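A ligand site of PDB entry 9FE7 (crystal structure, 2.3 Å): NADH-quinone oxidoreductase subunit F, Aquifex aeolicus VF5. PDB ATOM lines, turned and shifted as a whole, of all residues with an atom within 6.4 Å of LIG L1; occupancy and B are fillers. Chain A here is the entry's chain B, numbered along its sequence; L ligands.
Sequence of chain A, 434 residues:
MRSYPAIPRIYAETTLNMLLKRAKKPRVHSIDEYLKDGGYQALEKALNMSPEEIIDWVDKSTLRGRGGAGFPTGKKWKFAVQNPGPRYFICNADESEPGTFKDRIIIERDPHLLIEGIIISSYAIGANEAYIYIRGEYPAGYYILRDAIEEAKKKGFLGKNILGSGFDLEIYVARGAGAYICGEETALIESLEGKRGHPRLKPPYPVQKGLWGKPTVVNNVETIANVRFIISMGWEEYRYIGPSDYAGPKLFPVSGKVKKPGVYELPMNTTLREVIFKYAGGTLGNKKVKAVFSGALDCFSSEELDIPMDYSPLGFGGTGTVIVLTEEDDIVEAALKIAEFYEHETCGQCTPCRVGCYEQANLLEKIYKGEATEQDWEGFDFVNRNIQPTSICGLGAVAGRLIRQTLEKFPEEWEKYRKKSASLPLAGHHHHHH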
ATOM      1  N   ILE A 181     -17.417 -22.098  18.134  1.00  0.00           N
ATOM      2  CA  ILE A 181     -16.645 -23.049  18.915  1.00  0.00           C
ATOM      3  C   ILE A 181     -15.456 -22.352  19.586  1.00  0.00           C
ATOM      4  O   ILE A 181     -14.888 -22.883  20.535  1.00  0.00           O
ATOM      5  CB  ILE A 181     -16.207 -24.266  18.056  1.00  0.00           C
ATOM      6  CG1 ILE A 181     -15.758 -25.454  18.920  1.00  0.00           C
ATOM      7  CG2 ILE A 181     -15.131 -23.926  17.033  1.00  0.00           C
ATOM      8  CD1 ILE A 181     -16.815 -25.939  19.900  1.00  0.00           C
ATOM      9  N   GLY A 197      -9.895 -23.256  15.496  1.00  0.00           N
ATOM     10  CA  GLY A 197     -10.580 -23.448  16.764  1.00  0.00           C
ATOM     11  C   GLY A 197     -11.032 -24.894  16.979  1.00  0.00           C
ATOM     12  O   GLY A 197     -12.231 -25.186  16.911  1.00  0.00           O
ATOM     13  N   HIS A 198     -10.078 -25.791  17.260  1.00  0.00           N
ATOM     14  CA  HIS A 198     -10.378 -27.158  17.641  1.00  0.00           C
ATOM     15  C   HIS A 198     -10.203 -27.330  19.143  1.00  0.00           C
ATOM     16  O   HIS A 198      -9.089 -27.189  19.659  1.00  0.00           O
ATOM     17  CB  HIS A 198      -9.446 -28.154  16.935  1.00  0.00           C
ATOM     18  CG  HIS A 198      -9.678 -28.211  15.461  1.00  0.00           C
ATOM     19  ND1 HIS A 198      -8.688 -28.580  14.586  1.00  0.00           N
ATOM     20  CD2 HIS A 198     -10.759 -27.948  14.735  1.00  0.00           C
ATOM     21  CE1 HIS A 198      -9.185 -28.547  13.346  1.00  0.00           C
ATOM     22  NE2 HIS A 198     -10.437 -28.155  13.420  1.00  0.00           N
ATOM     23  N   PRO A 199     -11.277 -27.665  19.881  1.00  0.00           N
ATOM     24  CA  PRO A 199     -11.158 -27.975  21.309  1.00  0.00           C
ATOM     25  C   PRO A 199     -10.161 -29.105  21.564  1.00  0.00           C
ATOM     26  O   PRO A 199     -10.020 -30.020  20.752  1.00  0.00           O
ATOM     27  CB  PRO A 199     -12.582 -28.355  21.708  1.00  0.00           C
ATOM     28  CG  PRO A 199     -13.452 -27.651  20.704  1.00  0.00           C
ATOM     29  CD  PRO A 199     -12.663 -27.750  19.408  1.00  0.00           C
ATOM     30  N   ARG A 200      -9.444 -29.005  22.675  1.00  0.00           N
ATOM     31  CA  ARG A 200      -8.525 -30.039  23.094  1.00  0.00           C
ATOM     32  C   ARG A 200      -9.246 -31.032  24.015  1.00  0.00           C
ATOM     33  O   ARG A 200     -10.217 -30.698  24.684  1.00  0.00           O
ATOM     34  CB  ARG A 200      -7.389 -29.360  23.870  1.00  0.00           C
ATOM     35  CG  ARG A 200      -6.639 -28.251  23.145  1.00  0.00           C
ATOM     36  CD  ARG A 200      -5.991 -27.392  24.209  1.00  0.00           C
ATOM     37  NE  ARG A 200      -4.835 -26.629  23.734  1.00  0.00           N
ATOM     38  CZ  ARG A 200      -4.000 -25.890  24.474  1.00  0.00           C
ATOM     39  NH1 ARG A 200      -4.028 -25.933  25.795  1.00  0.00           N
ATOM     40  NH2 ARG A 200      -3.107 -25.134  23.864  1.00  0.00           N
ATOM     41  N   GLU A 345     -21.770 -24.967  13.248  1.00  0.00           N
ATOM     42  CA  GLU A 345     -20.805 -24.613  14.285  1.00  0.00           C
ATOM     43  C   GLU A 345     -19.975 -25.801  14.778  1.00  0.00           C
ATOM     44  O   GLU A 345     -18.967 -25.585  15.448  1.00  0.00           O
ATOM     45  CB  GLU A 345     -21.536 -23.888  15.413  1.00  0.00           C
ATOM     46  CG  GLU A 345     -22.085 -22.532  14.974  1.00  0.00           C
ATOM     47  CD  GLU A 345     -21.111 -21.585  14.285  1.00  0.00           C
ATOM     48  OE1 GLU A 345     -19.873 -21.724  14.354  1.00  0.00           O
ATOM     49  OE2 GLU A 345     -21.622 -20.650  13.638  1.00  0.00           O
ATOM     50  N   THR A 346     -20.366 -27.042  14.460  1.00  0.00           N
ATOM     51  CA  THR A 346     -19.518 -28.186  14.791  1.00  0.00           C
ATOM     52  C   THR A 346     -18.157 -28.026  14.126  1.00  0.00           C
ATOM     53  O   THR A 346     -18.078 -27.708  12.945  1.00  0.00           O
ATOM     54  CB  THR A 346     -20.179 -29.509  14.389  1.00  0.00           C
ATOM     55  OG1 THR A 346     -19.159 -30.471  14.617  1.00  0.00           O
ATOM     56  CG2 THR A 346     -20.581 -29.582  12.925  1.00  0.00           C
ATOM     57  N   CYS A 347     -17.086 -28.286  14.887  1.00  0.00           N
ATOM     58  CA  CYS A 347     -15.739 -28.173  14.369  1.00  0.00           C
ATOM     59  C   CYS A 347     -15.370 -29.399  13.531  1.00  0.00           C
ATOM     60  O   CYS A 347     -14.496 -29.311  12.670  1.00  0.00           O
ATOM     61  CB  CYS A 347     -14.760 -27.885  15.492  1.00  0.00           C
ATOM     62  SG  CYS A 347     -14.223 -29.346  16.417  1.00  0.00           S
ATOM     63  N   GLY A 348     -15.998 -30.545  13.805  1.00  0.00           N
ATOM     64  CA  GLY A 348     -15.876 -31.732  12.960  1.00  0.00           C
ATOM     65  C   GLY A 348     -14.880 -32.771  13.472  1.00  0.00           C
ATOM     66  O   GLY A 348     -14.786 -33.850  12.909  1.00  0.00           O
ATOM     67  N   GLN A 349     -14.108 -32.473  14.524  1.00  0.00           N
ATOM     68  CA  GLN A 349     -13.101 -33.419  14.973  1.00  0.00           C
ATOM     69  C   GLN A 349     -13.713 -34.768  15.350  1.00  0.00           C
ATOM     70  O   GLN A 349     -13.103 -35.785  15.093  1.00  0.00           O
ATOM     71  CB  GLN A 349     -12.404 -32.948  16.258  1.00  0.00           C
ATOM     72  CG  GLN A 349     -11.339 -31.892  16.045  1.00  0.00           C
ATOM     73  CD  GLN A 349     -10.881 -31.325  17.371  1.00  0.00           C
ATOM     74  OE1 GLN A 349     -11.617 -30.613  18.057  1.00  0.00           O
ATOM     75  NE2 GLN A 349      -9.670 -31.693  17.753  1.00  0.00           N
ATOM     76  N   CYS A 350     -14.868 -34.745  16.044  1.00  0.00           N
ATOM     77  CA  CYS A 350     -15.529 -35.958  16.496  1.00  0.00           C
ATOM     78  C   CYS A 350     -16.566 -36.396  15.447  1.00  0.00           C
ATOM     79  O   CYS A 350     -17.276 -35.552  14.900  1.00  0.00           O
ATOM     80  CB  CYS A 350     -16.146 -35.763  17.891  1.00  0.00           C
ATOM     81  SG  CYS A 350     -15.171 -34.742  19.032  1.00  0.00           S
ATOM     82  N   THR A 351     -16.665 -37.712  15.190  1.00  0.00           N
ATOM     83  CA  THR A 351     -17.461 -38.212  14.061  1.00  0.00           C
ATOM     84  C   THR A 351     -18.958 -38.033  14.341  1.00  0.00           C
ATOM     85  O   THR A 351     -19.670 -37.458  13.529  1.00  0.00           O
ATOM     86  CB  THR A 351     -17.084 -39.657  13.734  1.00  0.00           C
ATOM     87  OG1 THR A 351     -15.794 -39.592  13.122  1.00  0.00           O
ATOM     88  CG2 THR A 351     -18.015 -40.351  12.761  1.00  0.00           C
ATOM     89  N   CYS A 353     -20.556 -36.027  16.338  1.00  0.00           N
ATOM     90  CA  CYS A 353     -20.858 -34.605  16.304  1.00  0.00           C
ATOM     91  C   CYS A 353     -20.860 -34.116  14.849  1.00  0.00           C
ATOM     92  O   CYS A 353     -21.786 -33.431  14.417  1.00  0.00           O
ATOM     93  CB  CYS A 353     -19.897 -33.813  17.187  1.00  0.00           C
ATOM     94  SG  CYS A 353     -20.214 -32.026  17.277  1.00  0.00           S
ATOM     95  N   ARG A 354     -19.814 -34.457  14.104  1.00  0.00           N
ATOM     96  CA  ARG A 354     -19.631 -33.927  12.768  1.00  0.00           C
ATOM     97  C   ARG A 354     -20.849 -34.310  11.910  1.00  0.00           C
ATOM     98  O   ARG A 354     -21.474 -33.475  11.253  1.00  0.00           O
ATOM     99  CB  ARG A 354     -18.325 -34.468  12.180  1.00  0.00           C
ATOM    100  CG  ARG A 354     -18.137 -34.138  10.704  1.00  0.00           C
ATOM    101  CD  ARG A 354     -16.794 -34.618  10.140  1.00  0.00           C
ATOM    102  NE  ARG A 354     -16.760 -36.084  10.088  1.00  0.00           N
ATOM    103  CZ  ARG A 354     -16.132 -36.880  10.949  1.00  0.00           C
ATOM    104  NH1 ARG A 354     -15.531 -36.370  12.035  1.00  0.00           N
ATOM    105  NH2 ARG A 354     -16.114 -38.186  10.722  1.00  0.00           N
ATOM    106  N   CYS A 357     -24.634 -33.335  13.614  1.00  0.00           N
ATOM    107  CA  CYS A 357     -25.065 -31.947  13.483  1.00  0.00           C
ATOM    108  C   CYS A 357     -25.598 -31.743  12.067  1.00  0.00           C
ATOM    109  O   CYS A 357     -26.651 -31.126  11.879  1.00  0.00           O
ATOM    110  CB  CYS A 357     -23.967 -30.978  13.925  1.00  0.00           C
ATOM    111  SG  CYS A 357     -23.651 -30.920  15.713  1.00  0.00           S
ATOM    112  N   ILE A 387     -25.485 -37.702  18.813  1.00  0.00           N
ATOM    113  CA  ILE A 387     -24.492 -36.673  18.526  1.00  0.00           C
ATOM    114  C   ILE A 387     -23.377 -36.698  19.582  1.00  0.00           C
ATOM    115  O   ILE A 387     -22.216 -36.532  19.240  1.00  0.00           O
ATOM    116  CB  ILE A 387     -25.158 -35.298  18.446  1.00  0.00           C
ATOM    117  CG1 ILE A 387     -26.347 -35.320  17.459  1.00  0.00           C
ATOM    118  CG2 ILE A 387     -24.132 -34.225  18.086  1.00  0.00           C
ATOM    119  CD1 ILE A 387     -27.223 -34.074  17.442  1.00  0.00           C
ATOM    120  N   GLN A 388     -23.750 -36.930  20.852  1.00  0.00           N
ATOM    121  CA  GLN A 388     -22.860 -36.845  22.009  1.00  0.00           C
ATOM    122  C   GLN A 388     -21.735 -37.895  21.979  1.00  0.00           C
ATOM    123  O   GLN A 388     -20.605 -37.595  22.353  1.00  0.00           O
ATOM    124  CB  GLN A 388     -23.729 -36.967  23.271  1.00  0.00           C
ATOM    125  CG  GLN A 388     -22.975 -36.797  24.579  1.00  0.00           C
ATOM    126  CD  GLN A 388     -23.849 -36.432  25.764  1.00  0.00           C
ATOM    127  OE1 GLN A 388     -25.075 -36.333  25.688  1.00  0.00           O
ATOM    128  NE2 GLN A 388     -23.207 -36.193  26.896  1.00  0.00           N
ATOM    129  N   THR A 390     -18.551 -39.915  22.020  1.00  0.00           N
ATOM    130  CA  THR A 390     -17.148 -39.648  21.717  1.00  0.00           C
ATOM    131  C   THR A 390     -16.810 -38.148  21.713  1.00  0.00           C
ATOM    132  O   THR A 390     -15.666 -37.809  21.407  1.00  0.00           O
ATOM    133  CB  THR A 390     -16.717 -40.314  20.409  1.00  0.00           C
ATOM    134  OG1 THR A 390     -17.209 -39.579  19.292  1.00  0.00           O
ATOM    135  CG2 THR A 390     -17.150 -41.769  20.349  1.00  0.00           C
ATOM    136  N   SER A 391     -17.773 -37.268  22.055  1.00  0.00           N
ATOM    137  CA  SER A 391     -17.600 -35.823  22.112  1.00  0.00           C
ATOM    138  C   SER A 391     -16.432 -35.375  23.004  1.00  0.00           C
ATOM    139  O   SER A 391     -16.395 -35.729  24.176  1.00  0.00           O
ATOM    140  CB  SER A 391     -18.862 -35.152  22.597  1.00  0.00           C
ATOM    141  OG  SER A 391     -19.831 -35.127  21.576  1.00  0.00           O
ATOM    142  N   ILE A 392     -15.561 -34.509  22.439  1.00  0.00           N
ATOM    143  CA  ILE A 392     -14.472 -33.854  23.163  1.00  0.00           C
ATOM    144  C   ILE A 392     -14.984 -32.660  23.985  1.00  0.00           C
ATOM    145  O   ILE A 392     -14.327 -32.257  24.942  1.00  0.00           O
ATOM    146  CB  ILE A 392     -13.399 -33.298  22.205  1.00  0.00           C
ATOM    147  CG1 ILE A 392     -12.468 -34.322  21.638  1.00  0.00           C
ATOM    148  CG2 ILE A 392     -12.575 -32.193  22.880  1.00  0.00           C
ATOM    149  CD1 ILE A 392     -11.442 -33.695  20.706  1.00  0.00           C
ATOM    150  N   CYS A 393     -16.064 -32.013  23.543  1.00  0.00           N
ATOM    151  CA  CYS A 393     -16.505 -30.783  24.168  1.00  0.00           C
ATOM    152  C   CYS A 393     -18.028 -30.775  24.270  1.00  0.00           C
ATOM    153  O   CYS A 393     -18.703 -31.650  23.715  1.00  0.00           O
ATOM    154  CB  CYS A 393     -15.939 -29.560  23.439  1.00  0.00           C
ATOM    155  SG  CYS A 393     -16.922 -29.004  22.027  1.00  0.00           S
ATOM    156  N   GLY A 394     -18.565 -29.748  24.950  1.00  0.00           N
ATOM    157  CA  GLY A 394     -19.976 -29.696  25.316  1.00  0.00           C
ATOM    158  C   GLY A 394     -20.911 -29.484  24.127  1.00  0.00           C
ATOM    159  O   GLY A 394     -22.114 -29.701  24.258  1.00  0.00           O
ATOM    160  N   LEU A 395     -20.386 -29.062  22.966  1.00  0.00           N
ATOM    161  CA  LEU A 395     -21.240 -28.733  21.834  1.00  0.00           C
ATOM    162  C   LEU A 395     -21.971 -30.007  21.390  1.00  0.00           C
ATOM    163  O   LEU A 395     -23.175 -29.976  21.126  1.00  0.00           O
ATOM    164  CB  LEU A 395     -20.471 -28.108  20.677  1.00  0.00           C
ATOM    165  CG  LEU A 395     -21.330 -27.589  19.510  1.00  0.00           C
ATOM    166  CD1 LEU A 395     -20.659 -26.438  18.772  1.00  0.00           C
ATOM    167  CD2 LEU A 395     -21.643 -28.708  18.520  1.00  0.00           C
ATOM    168  N   GLY A 396     -21.232 -31.101  21.285  1.00  0.00           N
ATOM    169  CA  GLY A 396     -21.770 -32.358  20.792  1.00  0.00           C
ATOM    170  C   GLY A 396     -22.676 -32.979  21.848  1.00  0.00           C
ATOM    171  O   GLY A 396     -23.662 -33.629  21.519  1.00  0.00           O
ATOM    172  N   ALA A 397     -22.359 -32.703  23.127  1.00  0.00           N
ATOM    173  CA  ALA A 397     -23.203 -33.118  24.239  1.00  0.00           C
ATOM    174  C   ALA A 397     -24.574 -32.438  24.216  1.00  0.00           C
ATOM    175  O   ALA A 397     -25.540 -33.012  24.705  1.00  0.00           O
ATOM    176  CB  ALA A 397     -22.496 -32.849  25.542  1.00  0.00           C
HETATM  177 FE1  LIG L   1     -15.755 -30.291  17.687  1.00  0.00          FE
HETATM  178 FE2  LIG L   1     -18.242 -31.310  18.122  1.00  0.00          FE
HETATM  179 FE3  LIG L   1     -16.764 -30.308  20.202  1.00  0.00          FE
HETATM  180 FE4  LIG L   1     -16.034 -32.641  18.917  1.00  0.00          FE
HETATM  181  S1  LIG L   1     -17.956 -32.258  20.155  1.00  0.00           S
HETATM  182  S2  LIG L   1     -14.631 -30.946  19.529  1.00  0.00           S
HETATM  183  S3  LIG L   1     -16.603 -32.178  16.802  1.00  0.00           S
HETATM  184  S4  LIG L   1     -17.593 -29.166  18.400  1.00  0.00           S
HETATM  185  N1  LG2 L   2     -17.951 -19.061  27.578  1.00  0.00           N
HETATM  186  C1  LG2 L   2     -17.994 -17.684  27.371  1.00  0.00           C
HETATM  187  O1  LG2 L   2     -17.667 -16.868  28.249  1.00  0.00           O
HETATM  188  N2  LG2 L   2     -18.382 -17.183  26.162  1.00  0.00           N
HETATM  189  C2  LG2 L   2     -18.745 -17.929  25.062  1.00  0.00           C
HETATM  190  O2  LG2 L   2     -19.128 -17.353  24.053  1.00  0.00           O
HETATM  191  C3  LG2 L   2     -18.680 -19.377  25.258  1.00  0.00           C
HETATM  192  N3  LG2 L   2     -18.955 -20.146  24.244  1.00  0.00           N
HETATM  193  C4  LG2 L   2     -18.864 -21.518  24.433  1.00  0.00           C
HETATM  194  C5  LG2 L   2     -19.130 -22.351  23.348  1.00  0.00           C
HETATM  195  C6  LG2 L   2     -19.095 -23.733  23.478  1.00  0.00           C
HETATM  196  C7  LG2 L   2     -19.472 -24.600  22.303  1.00  0.00           C
HETATM  197  C8  LG2 L   2     -18.750 -24.302  24.718  1.00  0.00           C
HETATM  198  C9  LG2 L   2     -18.748 -25.803  24.912  1.00  0.00           C
HETATM  199  C10 LG2 L   2     -18.449 -23.469  25.790  1.00  0.00           C
HETATM  200  C11 LG2 L   2     -18.516 -22.082  25.665  1.00  0.00           C
HETATM  201  N4  LG2 L   2     -18.218 -21.201  26.752  1.00  0.00           N
HETATM  202  C12 LG2 L   2     -18.287 -19.846  26.559  1.00  0.00           C
HETATM  203  C13 LG2 L   2     -17.797 -21.693  28.060  1.00  0.00           C
HETATM  204  C14 LG2 L   2     -16.290 -21.644  28.227  1.00  0.00           C
HETATM  205  O3  LG2 L   2     -15.676 -22.811  27.656  1.00  0.00           O
HETATM  206  C15 LG2 L   2     -15.902 -21.513  29.708  1.00  0.00           C
HETATM  207  O4  LG2 L   2     -16.779 -22.301  30.508  1.00  0.00           O
HETATM  208  C16 LG2 L   2     -15.991 -20.093  30.256  1.00  0.00           C
HETATM  209  O5  LG2 L   2     -15.560 -19.146  29.287  1.00  0.00           O
HETATM  210  C17 LG2 L   2     -15.236 -19.954  31.557  1.00  0.00           C
HETATM  211  O6  LG2 L   2     -15.544 -18.666  32.126  1.00  0.00           O
HETATM  212  P1  LG2 L   2     -16.568 -18.572  33.334  1.00  0.00           P
HETATM  213  O7  LG2 L   2     -17.953 -18.762  32.884  1.00  0.00           O
HETATM  214  O8  LG2 L   2     -16.103 -19.523  34.378  1.00  0.00           O
HETATM  215  O9  LG2 L   2     -16.297 -17.143  33.868  1.00  0.00           O
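Merely in contact with LIG L1: Ile 181 (3.6 Å), Pro 199 (3.7 Å), Ile 392 (3.8 Å) and Leu 395 (3.8 Å). Hydrophobic or aromatic side chains that line LIG L1: Ile 181, Pro 199, Ile 392 and Leu 395. Of the 25 residues printed, 13 come within 4 Å of LIG L1. The nearest printed residue that does not touch LIG L1 is Arg 354 (4.8 Å).
The backbone NH (N) of Cys 347 sits close to a sulfur (S4) of LIG L1 (3.7 Å). The side-chain sulfur (SG) of Cys 347 is bound to an iron atom (FE1) of LIG L1. FE3 of LIG L1 is bound by SG of Cys 393. The side-chain sulfur (SG) of Cys 353 is bound to an iron atom (FE2) of LIG L1 (2.3 Å). The backbone NH of Cys 350 sits close to a sulfur (S3) of LIG L1 (3.2 Å). An iron atom (FE4) of LIG L1 is bound by the side-chain sulfur (SG) of Cys 350, 2.3 Å away. The backbone NH of Gln 349 lies close to a sulfur (S3) of LIG L1 (3.4 Å). The side-chain amide oxygen (OE1) of Gln 349 lies close to a sulfur (S2) of LIG L1, 3.4 Å away. The backbone NH of Gly 348 sits close to a sulfur (S3) of LIG L1. N of Gly 396 lies close to S1 of LIG L1, 3.7 Å away. S1 of LIG L1 sits close to OG of Ser 391, 3.7 Å away. The side-chain hydroxyl of Thr 346 sits close to a sulfur (S3) of LIG L1, at 3.8 Å.
SG of Cys 347 sits close to OE1 of Gln 349 (3.3 Å). SG of Cys 357 sits close to O of Cys 353 (3.4 Å). The backbone carbonyl oxygen of Cys 350 sits close to the guanidinium group of Arg 354 (3.5 Å). The backbone carbonyl oxygen (O) of Pro 199 lies close to the side-chain amide oxygen (OE1) of Gln 349 (3.2 Å). The backbone NH of Gly 348 sits at hydrogen-bond distance from the side-chain hydroxyl of Thr 346, 3.3 Å away. O of Gly 348 sits at hydrogen-bond distance from NH1 of Arg 354, at 2.8 Å. The backbone carbonyl oxygen (O) of Gly 396 lies close to the backbone NH (N) of Gln 388, 3.4 Å away. OG of Ser 391 sits at hydrogen-bond distance from O of Gln 388 (2.7 Å).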
